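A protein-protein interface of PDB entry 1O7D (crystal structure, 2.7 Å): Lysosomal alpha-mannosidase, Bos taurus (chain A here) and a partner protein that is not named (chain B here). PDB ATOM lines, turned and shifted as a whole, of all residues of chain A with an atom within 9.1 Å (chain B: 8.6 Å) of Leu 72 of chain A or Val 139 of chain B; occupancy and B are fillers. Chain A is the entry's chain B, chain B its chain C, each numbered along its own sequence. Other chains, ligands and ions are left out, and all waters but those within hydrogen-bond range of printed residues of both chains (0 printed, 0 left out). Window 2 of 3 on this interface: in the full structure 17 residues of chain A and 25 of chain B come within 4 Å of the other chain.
Of the printed residues of chain B, Gln 68 of chain A touches Tyr 85 (3.0 Å) and Pro 87 (3.1 Å). No residue of chain B comes within 4 Å of Ala 71 of chain A. Leu 72 of chain A touches just these residues of chain B: Tyr 85 and Val 139. No residue of chain B comes within 4 Å of Ala 73 of chain A. Printed residues of chain A within 4 Å of Leu 50 of chain B: Leu 69 (3.997 Å). Ala 138 of chain B touches none of the printed residues of chain A. Val 139 of chain B touches one residue of chain A. No residue of chain A comes within 4 Å of Gly 140 of chain B. The nearest residue of chain B that does not touch Leu 72 of chain A is Leu 53 of chain B (4.2 Å). The nearest residue of chain A that does not touch Val 139 of chain B is Gln 68 of chain A (4.4 Å). The nearest printed residue of chain B that does not touch Gln 68 of chain A is Asn 86 of chain B (4.3 Å).
Of the 20 printed residues of chain B, 5 touch a printed residue of chain A. Hydrophobic or aromatic side chains of chain B that line the printed part of chain A: Ala 49, Leu 50, Tyr 85, Pro 87 and Val 139. Of the 12 printed residues of chain A, 4 touch a printed residue of chain B. Among the printed residues, 9 pairs touch across the chains. Among the printed residues, no Asp or Glu carboxylate lies within 4 Å of a Lys or Arg side-chain nitrogen of the other chain.
Val 65 of chain A touches Tyr 85 of chain B. Val 65 of chain A touches Pro 87 of chain B (CG2 to CG, 3.2 Å). Leu 69 of chain A touches Ala 49 of chain B (CB to CB, 3.7 Å). Leu 69 of chain A touches Leu 50 of chain B. CD2 of Leu 69 of chain A touches CE2 of Tyr 85 of chain B (3.3 Å). Leu 72 of chain A touches Tyr 85 of chain B (CD1 to OH, 3.6 Å). CD1 of Leu 72 of chain A touches O of Val 139 of chain B, at 3.8 Å.
The backbone carbonyl oxygen (O) of Asn 86 of chain B sits at hydrogen-bond distance from the backbone NH (N) of Val 139 of chain B (3.2 Å). The backbone NH (N) of Val 139 of chain B is in hydrogen-bond range of the backbone carbonyl oxygen (O) of Leu 88 of chain B, 3.1 Å away.
OH of Tyr 85 of chain B is in hydrogen-bond range of OE1 of Gln 68 of chain A, at 3.0 Å. The backbone carbonyl oxygen (O) of Pro 87 of chain B lies within hydrogen-bond range of the side-chain amide nitrogen (NE2) of Gln 68 of chain A (3.1 Å).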
ATOM      1  N   GLN A  64       3.452   0.540  34.289  1.00  0.00           N
ATOM      2  CA  GLN A  64       3.688   1.927  33.923  1.00  0.00           C
ATOM      3  C   GLN A  64       3.111   2.215  32.548  1.00  0.00           C
ATOM      4  O   GLN A  64       2.294   3.116  32.381  1.00  0.00           O
ATOM      5  CB  GLN A  64       5.181   2.206  33.894  1.00  0.00           C
ATOM      6  CG  GLN A  64       5.534   3.470  34.599  1.00  0.00           C
ATOM      7  CD  GLN A  64       5.500   3.304  36.095  1.00  0.00           C
ATOM      8  OE1 GLN A  64       4.568   2.709  36.658  1.00  0.00           O
ATOM      9  NE2 GLN A  64       6.520   3.839  36.759  1.00  0.00           N
ATOM     10  N   VAL A  65       3.572   1.453  31.565  1.00  0.00           N
ATOM     11  CA  VAL A  65       3.102   1.586  30.205  1.00  0.00           C
ATOM     12  C   VAL A  65       1.593   1.476  30.225  1.00  0.00           C
ATOM     13  O   VAL A  65       0.907   2.230  29.564  1.00  0.00           O
ATOM     14  CB  VAL A  65       3.691   0.471  29.331  1.00  0.00           C
ATOM     15  CG1 VAL A  65       3.085   0.505  27.956  1.00  0.00           C
ATOM     16  CG2 VAL A  65       5.211   0.632  29.250  1.00  0.00           C
ATOM     17  N   CYS A  66       1.077   0.536  31.004  1.00  0.00           N
ATOM     18  CA  CYS A  66      -0.367   0.343  31.127  1.00  0.00           C
ATOM     19  C   CYS A  66      -0.993   1.642  31.646  1.00  0.00           C
ATOM     20  O   CYS A  66      -1.966   2.133  31.077  1.00  0.00           O
ATOM     21  CB  CYS A  66      -0.668  -0.829  32.087  1.00  0.00           C
ATOM     22  SG  CYS A  66      -2.419  -1.382  32.288  1.00  0.00           S
ATOM     23  N   ASN A  67      -0.425   2.200  32.715  1.00  0.00           N
ATOM     24  CA  ASN A  67      -0.929   3.443  33.288  1.00  0.00           C
ATOM     25  C   ASN A  67      -0.924   4.582  32.287  1.00  0.00           C
ATOM     26  O   ASN A  67      -1.949   5.231  32.078  1.00  0.00           O
ATOM     27  CB  ASN A  67      -0.097   3.864  34.498  1.00  0.00           C
ATOM     28  CG  ASN A  67      -0.489   3.127  35.748  1.00  0.00           C
ATOM     29  OD1 ASN A  67      -1.678   2.940  36.016  1.00  0.00           O
ATOM     30  ND2 ASN A  67       0.501   2.710  36.529  1.00  0.00           N
ATOM     31  N   GLN A  68       0.233   4.830  31.674  1.00  0.00           N
ATOM     32  CA  GLN A  68       0.360   5.911  30.709  1.00  0.00           C
ATOM     33  C   GLN A  68      -0.659   5.812  29.595  1.00  0.00           C
ATOM     34  O   GLN A  68      -1.167   6.826  29.156  1.00  0.00           O
ATOM     35  CB  GLN A  68       1.748   5.943  30.079  1.00  0.00           C
ATOM     36  CG  GLN A  68       2.902   6.212  31.006  1.00  0.00           C
ATOM     37  CD  GLN A  68       4.154   6.683  30.250  1.00  0.00           C
ATOM     38  OE1 GLN A  68       4.317   6.428  29.051  1.00  0.00           O
ATOM     39  NE2 GLN A  68       5.043   7.362  30.956  1.00  0.00           N
ATOM     40  N   LEU A  69      -0.965   4.607  29.123  1.00  0.00           N
ATOM     41  CA  LEU A  69      -1.935   4.486  28.034  1.00  0.00           C
ATOM     42  C   LEU A  69      -3.383   4.748  28.455  1.00  0.00           C
ATOM     43  O   LEU A  69      -4.180   5.301  27.684  1.00  0.00           O
ATOM     44  CB  LEU A  69      -1.834   3.108  27.369  1.00  0.00           C
ATOM     45  CG  LEU A  69      -0.743   2.985  26.307  1.00  0.00           C
ATOM     46  CD1 LEU A  69      -0.804   1.606  25.692  1.00  0.00           C
ATOM     47  CD2 LEU A  69      -0.933   4.054  25.250  1.00  0.00           C
ATOM     48  N   GLU A  70      -3.715   4.339  29.675  1.00  0.00           N
ATOM     49  CA  GLU A  70      -5.049   4.527  30.219  1.00  0.00           C
ATOM     50  C   GLU A  70      -5.262   6.032  30.370  1.00  0.00           C
ATOM     51  O   GLU A  70      -6.370   6.534  30.210  1.00  0.00           O
ATOM     52  CB  GLU A  70      -5.131   3.827  31.578  1.00  0.00           C
ATOM     53  CG  GLU A  70      -6.495   3.819  32.252  1.00  0.00           C
ATOM     54  CD  GLU A  70      -6.475   3.074  33.597  1.00  0.00           C
ATOM     55  OE1 GLU A  70      -5.569   3.338  34.422  1.00  0.00           O
ATOM     56  OE2 GLU A  70      -7.366   2.225  33.837  1.00  0.00           O
ATOM     57  N   ALA A  71      -4.177   6.745  30.660  1.00  0.00           N
ATOM     58  CA  ALA A  71      -4.218   8.188  30.845  1.00  0.00           C
ATOM     59  C   ALA A  71      -4.408   8.929  29.534  1.00  0.00           C
ATOM     60  O   ALA A  71      -5.164   9.893  29.459  1.00  0.00           O
ATOM     61  CB  ALA A  71      -2.931   8.660  31.533  1.00  0.00           C
ATOM     62  N   LEU A  72      -3.711   8.481  28.500  1.00  0.00           N
ATOM     63  CA  LEU A  72      -3.810   9.104  27.185  1.00  0.00           C
ATOM     64  C   LEU A  72      -5.166   8.850  26.492  1.00  0.00           C
ATOM     65  O   LEU A  72      -5.648   9.699  25.742  1.00  0.00           O
ATOM     66  CB  LEU A  72      -2.647   8.627  26.310  1.00  0.00           C
ATOM     67  CG  LEU A  72      -1.275   8.917  26.925  1.00  0.00           C
ATOM     68  CD1 LEU A  72      -0.164   8.394  26.027  1.00  0.00           C
ATOM     69  CD2 LEU A  72      -1.135  10.402  27.148  1.00  0.00           C
ATOM     70  N   ALA A  73      -5.785   7.695  26.736  1.00  0.00           N
ATOM     71  CA  ALA A  73      -7.101   7.406  26.146  1.00  0.00           C
ATOM     72  C   ALA A  73      -8.174   7.920  27.113  1.00  0.00           C
ATOM     73  O   ALA A  73      -7.960   7.901  28.330  1.00  0.00           O
ATOM     74  CB  ALA A  73      -7.263   5.904  25.934  1.00  0.00           C
ATOM     75  N   GLY A  74      -9.323   8.373  26.611  1.00  0.00           N
ATOM     76  CA  GLY A  74     -10.333   8.873  27.545  1.00  0.00           C
ATOM     77  C   GLY A  74     -11.678   8.156  27.595  1.00  0.00           C
ATOM     78  O   GLY A  74     -12.709   8.814  27.383  1.00  0.00           O
ATOM     79  N   PRO A  75     -11.722   6.837  27.903  1.00  0.00           N
ATOM     80  CA  PRO A  75     -12.983   6.076  27.960  1.00  0.00           C
ATOM     81  C   PRO A  75     -14.073   6.698  28.857  1.00  0.00           C
ATOM     82  O   PRO A  75     -15.037   5.951  29.207  1.00  0.00           O
ATOM     83  CB  PRO A  75     -12.543   4.694  28.468  1.00  0.00           C
ATOM     84  CG  PRO A  75     -11.123   4.589  27.974  1.00  0.00           C
ATOM     85  CD  PRO A  75     -10.587   5.979  28.292  1.00  0.00           C
ATOM     86  N   ALA B  49      -6.724   1.190  24.314  1.00  0.00           N
ATOM     87  CA  ALA B  49      -5.984   2.437  24.257  1.00  0.00           C
ATOM     88  C   ALA B  49      -5.423   2.688  22.860  1.00  0.00           C
ATOM     89  O   ALA B  49      -5.662   3.741  22.263  1.00  0.00           O
ATOM     90  CB  ALA B  49      -4.849   2.420  25.287  1.00  0.00           C
ATOM     91  N   LEU B  50      -4.682   1.712  22.340  1.00  0.00           N
ATOM     92  CA  LEU B  50      -4.066   1.820  21.019  1.00  0.00           C
ATOM     93  C   LEU B  50      -5.076   1.890  19.892  1.00  0.00           C
ATOM     94  O   LEU B  50      -4.981   2.759  19.021  1.00  0.00           O
ATOM     95  CB  LEU B  50      -3.146   0.639  20.762  1.00  0.00           C
ATOM     96  CG  LEU B  50      -2.008   0.457  21.762  1.00  0.00           C
ATOM     97  CD1 LEU B  50      -1.295  -0.856  21.458  1.00  0.00           C
ATOM     98  CD2 LEU B  50      -1.050   1.636  21.703  1.00  0.00           C
ATOM     99  N   HIS B  52      -7.887   2.972  19.932  1.00  0.00           N
ATOM    100  CA  HIS B  52      -8.410   4.328  19.956  1.00  0.00           C
ATOM    101  C   HIS B  52      -7.383   5.321  19.412  1.00  0.00           C
ATOM    102  O   HIS B  52      -7.667   6.081  18.489  1.00  0.00           O
ATOM    103  CB  HIS B  52      -8.823   4.726  21.379  1.00  0.00           C
ATOM    104  CG  HIS B  52      -9.409   6.101  21.470  1.00  0.00           C
ATOM    105  ND1 HIS B  52     -10.654   6.417  20.963  1.00  0.00           N
ATOM    106  CD2 HIS B  52      -8.902   7.256  21.964  1.00  0.00           C
ATOM    107  CE1 HIS B  52     -10.884   7.706  21.141  1.00  0.00           C
ATOM    108  NE2 HIS B  52      -9.837   8.240  21.744  1.00  0.00           N
ATOM    109  N   LEU B  53      -6.179   5.308  19.962  1.00  0.00           N
ATOM    110  CA  LEU B  53      -5.167   6.243  19.503  1.00  0.00           C
ATOM    111  C   LEU B  53      -4.701   6.120  18.037  1.00  0.00           C
ATOM    112  O   LEU B  53      -4.348   7.129  17.428  1.00  0.00           O
ATOM    113  CB  LEU B  53      -3.963   6.183  20.445  1.00  0.00           C
ATOM    114  CG  LEU B  53      -4.251   6.643  21.875  1.00  0.00           C
ATOM    115  CD1 LEU B  53      -3.050   6.383  22.745  1.00  0.00           C
ATOM    116  CD2 LEU B  53      -4.593   8.114  21.883  1.00  0.00           C
ATOM    117  N   VAL B  84       5.641  -0.344  18.734  1.00  0.00           N
ATOM    118  CA  VAL B  84       6.576  -0.182  19.843  1.00  0.00           C
ATOM    119  C   VAL B  84       6.253   1.080  20.643  1.00  0.00           C
ATOM    120  O   VAL B  84       6.372   2.183  20.123  1.00  0.00           O
ATOM    121  CB  VAL B  84       8.029  -0.099  19.342  1.00  0.00           C
ATOM    122  CG1 VAL B  84       8.974  -0.061  20.501  1.00  0.00           C
ATOM    123  CG2 VAL B  84       8.345  -1.291  18.491  1.00  0.00           C
ATOM    124  N   TYR B  85       5.840   0.910  21.899  1.00  0.00           N
ATOM    125  CA  TYR B  85       5.504   2.040  22.778  1.00  0.00           C
ATOM    126  C   TYR B  85       6.691   2.431  23.639  1.00  0.00           C
ATOM    127  O   TYR B  85       7.391   1.567  24.157  1.00  0.00           O
ATOM    128  CB  TYR B  85       4.327   1.693  23.699  1.00  0.00           C
ATOM    129  CG  TYR B  85       3.837   2.860  24.538  1.00  0.00           C
ATOM    130  CD1 TYR B  85       4.486   3.228  25.715  1.00  0.00           C
ATOM    131  CD2 TYR B  85       2.734   3.611  24.129  1.00  0.00           C
ATOM    132  CE1 TYR B  85       4.047   4.314  26.463  1.00  0.00           C
ATOM    133  CE2 TYR B  85       2.285   4.698  24.860  1.00  0.00           C
ATOM    134  CZ  TYR B  85       2.940   5.053  26.027  1.00  0.00           C
ATOM    135  OH  TYR B  85       2.499   6.152  26.735  1.00  0.00           O
ATOM    136  N   ASN B  86       6.900   3.737  23.795  1.00  0.00           N
ATOM    137  CA  ASN B  86       7.998   4.263  24.595  1.00  0.00           C
ATOM    138  C   ASN B  86       7.466   5.109  25.743  1.00  0.00           C
ATOM    139  O   ASN B  86       6.815   6.126  25.523  1.00  0.00           O
ATOM    140  CB  ASN B  86       8.921   5.092  23.709  1.00  0.00           C
ATOM    141  CG  ASN B  86       9.894   5.923  24.497  1.00  0.00           C
ATOM    142  OD1 ASN B  86      10.435   5.488  25.497  1.00  0.00           O
ATOM    143  ND2 ASN B  86      10.136   7.126  24.033  1.00  0.00           N
ATOM    144  N   PRO B  87       7.724   4.688  26.986  1.00  0.00           N
ATOM    145  CA  PRO B  87       7.291   5.375  28.205  1.00  0.00           C
ATOM    146  C   PRO B  87       8.162   6.553  28.654  1.00  0.00           C
ATOM    147  O   PRO B  87       7.763   7.294  29.546  1.00  0.00           O
ATOM    148  CB  PRO B  87       7.304   4.266  29.251  1.00  0.00           C
ATOM    149  CG  PRO B  87       7.240   3.030  28.459  1.00  0.00           C
ATOM    150  CD  PRO B  87       8.131   3.319  27.309  1.00  0.00           C
ATOM    151  N   LEU B  88       9.341   6.723  28.059  1.00  0.00           N
ATOM    152  CA  LEU B  88      10.249   7.794  28.447  1.00  0.00           C
ATOM    153  C   LEU B  88       9.887   9.161  27.906  1.00  0.00           C
ATOM    154  O   LEU B  88       9.304   9.275  26.839  1.00  0.00           O
ATOM    155  CB  LEU B  88      11.677   7.444  28.044  1.00  0.00           C
ATOM    156  CG  LEU B  88      12.390   6.430  28.946  1.00  0.00           C
ATOM    157  CD1 LEU B  88      13.751   6.093  28.372  1.00  0.00           C
ATOM    158  CD2 LEU B  88      12.551   7.016  30.342  1.00  0.00           C
ATOM    159  N   GLY B  89      10.242  10.199  28.658  1.00  0.00           N
ATOM    160  CA  GLY B  89       9.935  11.564  28.266  1.00  0.00           C
ATOM    161  C   GLY B  89      10.797  12.109  27.148  1.00  0.00           C
ATOM    162  O   GLY B  89      10.900  13.321  26.973  1.00  0.00           O
ATOM    163  N   ARG B  90      11.425  11.213  26.394  1.00  0.00           N
ATOM    164  CA  ARG B  90      12.270  11.585  25.264  1.00  0.00           C
ATOM    165  C   ARG B  90      12.173  10.477  24.228  1.00  0.00           C
ATOM    166  O   ARG B  90      11.643   9.405  24.502  1.00  0.00           O
ATOM    167  CB  ARG B  90      13.709  11.792  25.719  1.00  0.00           C
ATOM    168  CG  ARG B  90      13.840  13.015  26.614  1.00  0.00           C
ATOM    169  CD  ARG B  90      15.202  13.125  27.280  1.00  0.00           C
ATOM    170  NE  ARG B  90      15.330  12.164  28.371  1.00  0.00           N
ATOM    171  CZ  ARG B  90      14.578  12.182  29.464  1.00  0.00           C
ATOM    172  NH1 ARG B  90      13.655  13.118  29.607  1.00  0.00           N
ATOM    173  NH2 ARG B  90      14.729  11.250  30.402  1.00  0.00           N
ATOM    174  N   LYS B  91      12.673  10.742  23.030  1.00  0.00           N
ATOM    175  CA  LYS B  91      12.596   9.778  21.941  1.00  0.00           C
ATOM    176  C   LYS B  91      13.550   8.610  22.158  1.00  0.00           C
ATOM    177  O   LYS B  91      14.597   8.756  22.797  1.00  0.00           O
ATOM    178  CB  LYS B  91      12.923  10.484  20.619  1.00  0.00           C
ATOM    179  CG  LYS B  91      14.342  11.063  20.607  1.00  0.00           C
ATOM    180  CD  LYS B  91      14.578  12.076  19.484  1.00  0.00           C
ATOM    181  CE  LYS B  91      15.998  12.687  19.602  1.00  0.00           C
ATOM    182  NZ  LYS B  91      16.388  13.694  18.545  1.00  0.00           N
ATOM    183  N   VAL B  92      13.175   7.449  21.629  1.00  0.00           N
ATOM    184  CA  VAL B  92      14.018   6.260  21.724  1.00  0.00           C
ATOM    185  C   VAL B  92      14.335   5.756  20.322  1.00  0.00           C
ATOM    186  O   VAL B  92      13.525   5.885  19.401  1.00  0.00           O
ATOM    187  CB  VAL B  92      13.337   5.110  22.530  1.00  0.00           C
ATOM    188  CG1 VAL B  92      14.092   3.811  22.323  1.00  0.00           C
ATOM    189  CG2 VAL B  92      13.334   5.449  24.017  1.00  0.00           C
ATOM    190  N   VAL B 136      11.081   5.824  18.296  1.00  0.00           N
ATOM    191  CA  VAL B 136       9.832   6.120  18.983  1.00  0.00           C
ATOM    192  C   VAL B 136       9.835   7.438  19.756  1.00  0.00           C
ATOM    193  O   VAL B 136      10.778   7.745  20.497  1.00  0.00           O
ATOM    194  CB  VAL B 136       9.477   4.992  19.953  1.00  0.00           C
ATOM    195  CG1 VAL B 136       8.101   5.226  20.547  1.00  0.00           C
ATOM    196  CG2 VAL B 136       9.522   3.666  19.228  1.00  0.00           C
ATOM    197  N   PRO B 137       8.763   8.232  19.598  1.00  0.00           N
ATOM    198  CA  PRO B 137       8.607   9.527  20.265  1.00  0.00           C
ATOM    199  C   PRO B 137       8.391   9.352  21.761  1.00  0.00           C
ATOM    200  O   PRO B 137       7.950   8.292  22.214  1.00  0.00           O
ATOM    201  CB  PRO B 137       7.368  10.115  19.596  1.00  0.00           C
ATOM    202  CG  PRO B 137       7.302   9.411  18.287  1.00  0.00           C
ATOM    203  CD  PRO B 137       7.654   8.006  18.660  1.00  0.00           C
ATOM    204  N   ALA B 138       8.693  10.391  22.526  1.00  0.00           N
ATOM    205  CA  ALA B 138       8.502  10.333  23.965  1.00  0.00           C
ATOM    206  C   ALA B 138       7.009  10.155  24.266  1.00  0.00           C
ATOM    207  O   ALA B 138       6.159  10.749  23.602  1.00  0.00           O
ATOM    208  CB  ALA B 138       9.026  11.605  24.602  1.00  0.00           C
ATOM    209  N   VAL B 139       6.701   9.313  25.248  1.00  0.00           N
ATOM    210  CA  VAL B 139       5.319   9.054  25.644  1.00  0.00           C
ATOM    211  C   VAL B 139       4.462   8.667  24.447  1.00  0.00           C
ATOM    212  O   VAL B 139       3.256   8.878  24.453  1.00  0.00           O
ATOM    213  CB  VAL B 139       4.695  10.291  26.306  1.00  0.00           C
ATOM    214  CG1 VAL B 139       3.294   9.992  26.766  1.00  0.00           C
ATOM    215  CG2 VAL B 139       5.524  10.714  27.488  1.00  0.00           C
ATOM    216  N   GLY B 140       5.089   8.101  23.416  1.00  0.00           N
ATOM    217  CA  GLY B 140       4.348   7.697  22.232  1.00  0.00           C
ATOM    218  C   GLY B 140       4.623   6.290  21.718  1.00  0.00           C
ATOM    219  O   GLY B 140       5.004   5.384  22.460  1.00  0.00           O
ATOM    220  N   PHE B 141       4.416   6.114  20.418  1.00  0.00           N
ATOM    221  CA  PHE B 141       4.627   4.835  19.773  1.00  0.00           C
ATOM    222  C   PHE B 141       4.817   4.986  18.270  1.00  0.00           C
ATOM    223  O   PHE B 141       4.530   6.041  17.682  1.00  0.00           O
ATOM    224  CB  PHE B 141       3.434   3.919  20.035  1.00  0.00           C
ATOM    225  CG  PHE B 141       2.115   4.461  19.536  1.00  0.00           C
ATOM    226  CD1 PHE B 141       1.899   4.689  18.183  1.00  0.00           C
ATOM    227  CD2 PHE B 141       1.079   4.714  20.422  1.00  0.00           C
ATOM    228  CE1 PHE B 141       0.673   5.154  17.724  1.00  0.00           C
ATOM    229  CE2 PHE B 141      -0.149   5.178  19.972  1.00  0.00           C
ATOM    230  CZ  PHE B 141      -0.352   5.400  18.621  1.00  0.00           C
ATOM    231  N   SER B 142       5.286   3.909  17.654  1.00  0.00           N
ATOM    232  CA  SER B 142       5.511   3.861  16.214  1.00  0.00           C
ATOM    233  C   SER B 142       5.034   2.511  15.703  1.00  0.00           C
ATOM    234  O   SER B 142       5.136   1.500  16.399  1.00  0.00           O
ATOM    235  CB  SER B 142       6.996   4.012  15.886  1.00  0.00           C
ATOM    236  OG  SER B 142       7.442   5.324  16.137  1.00  0.00           O
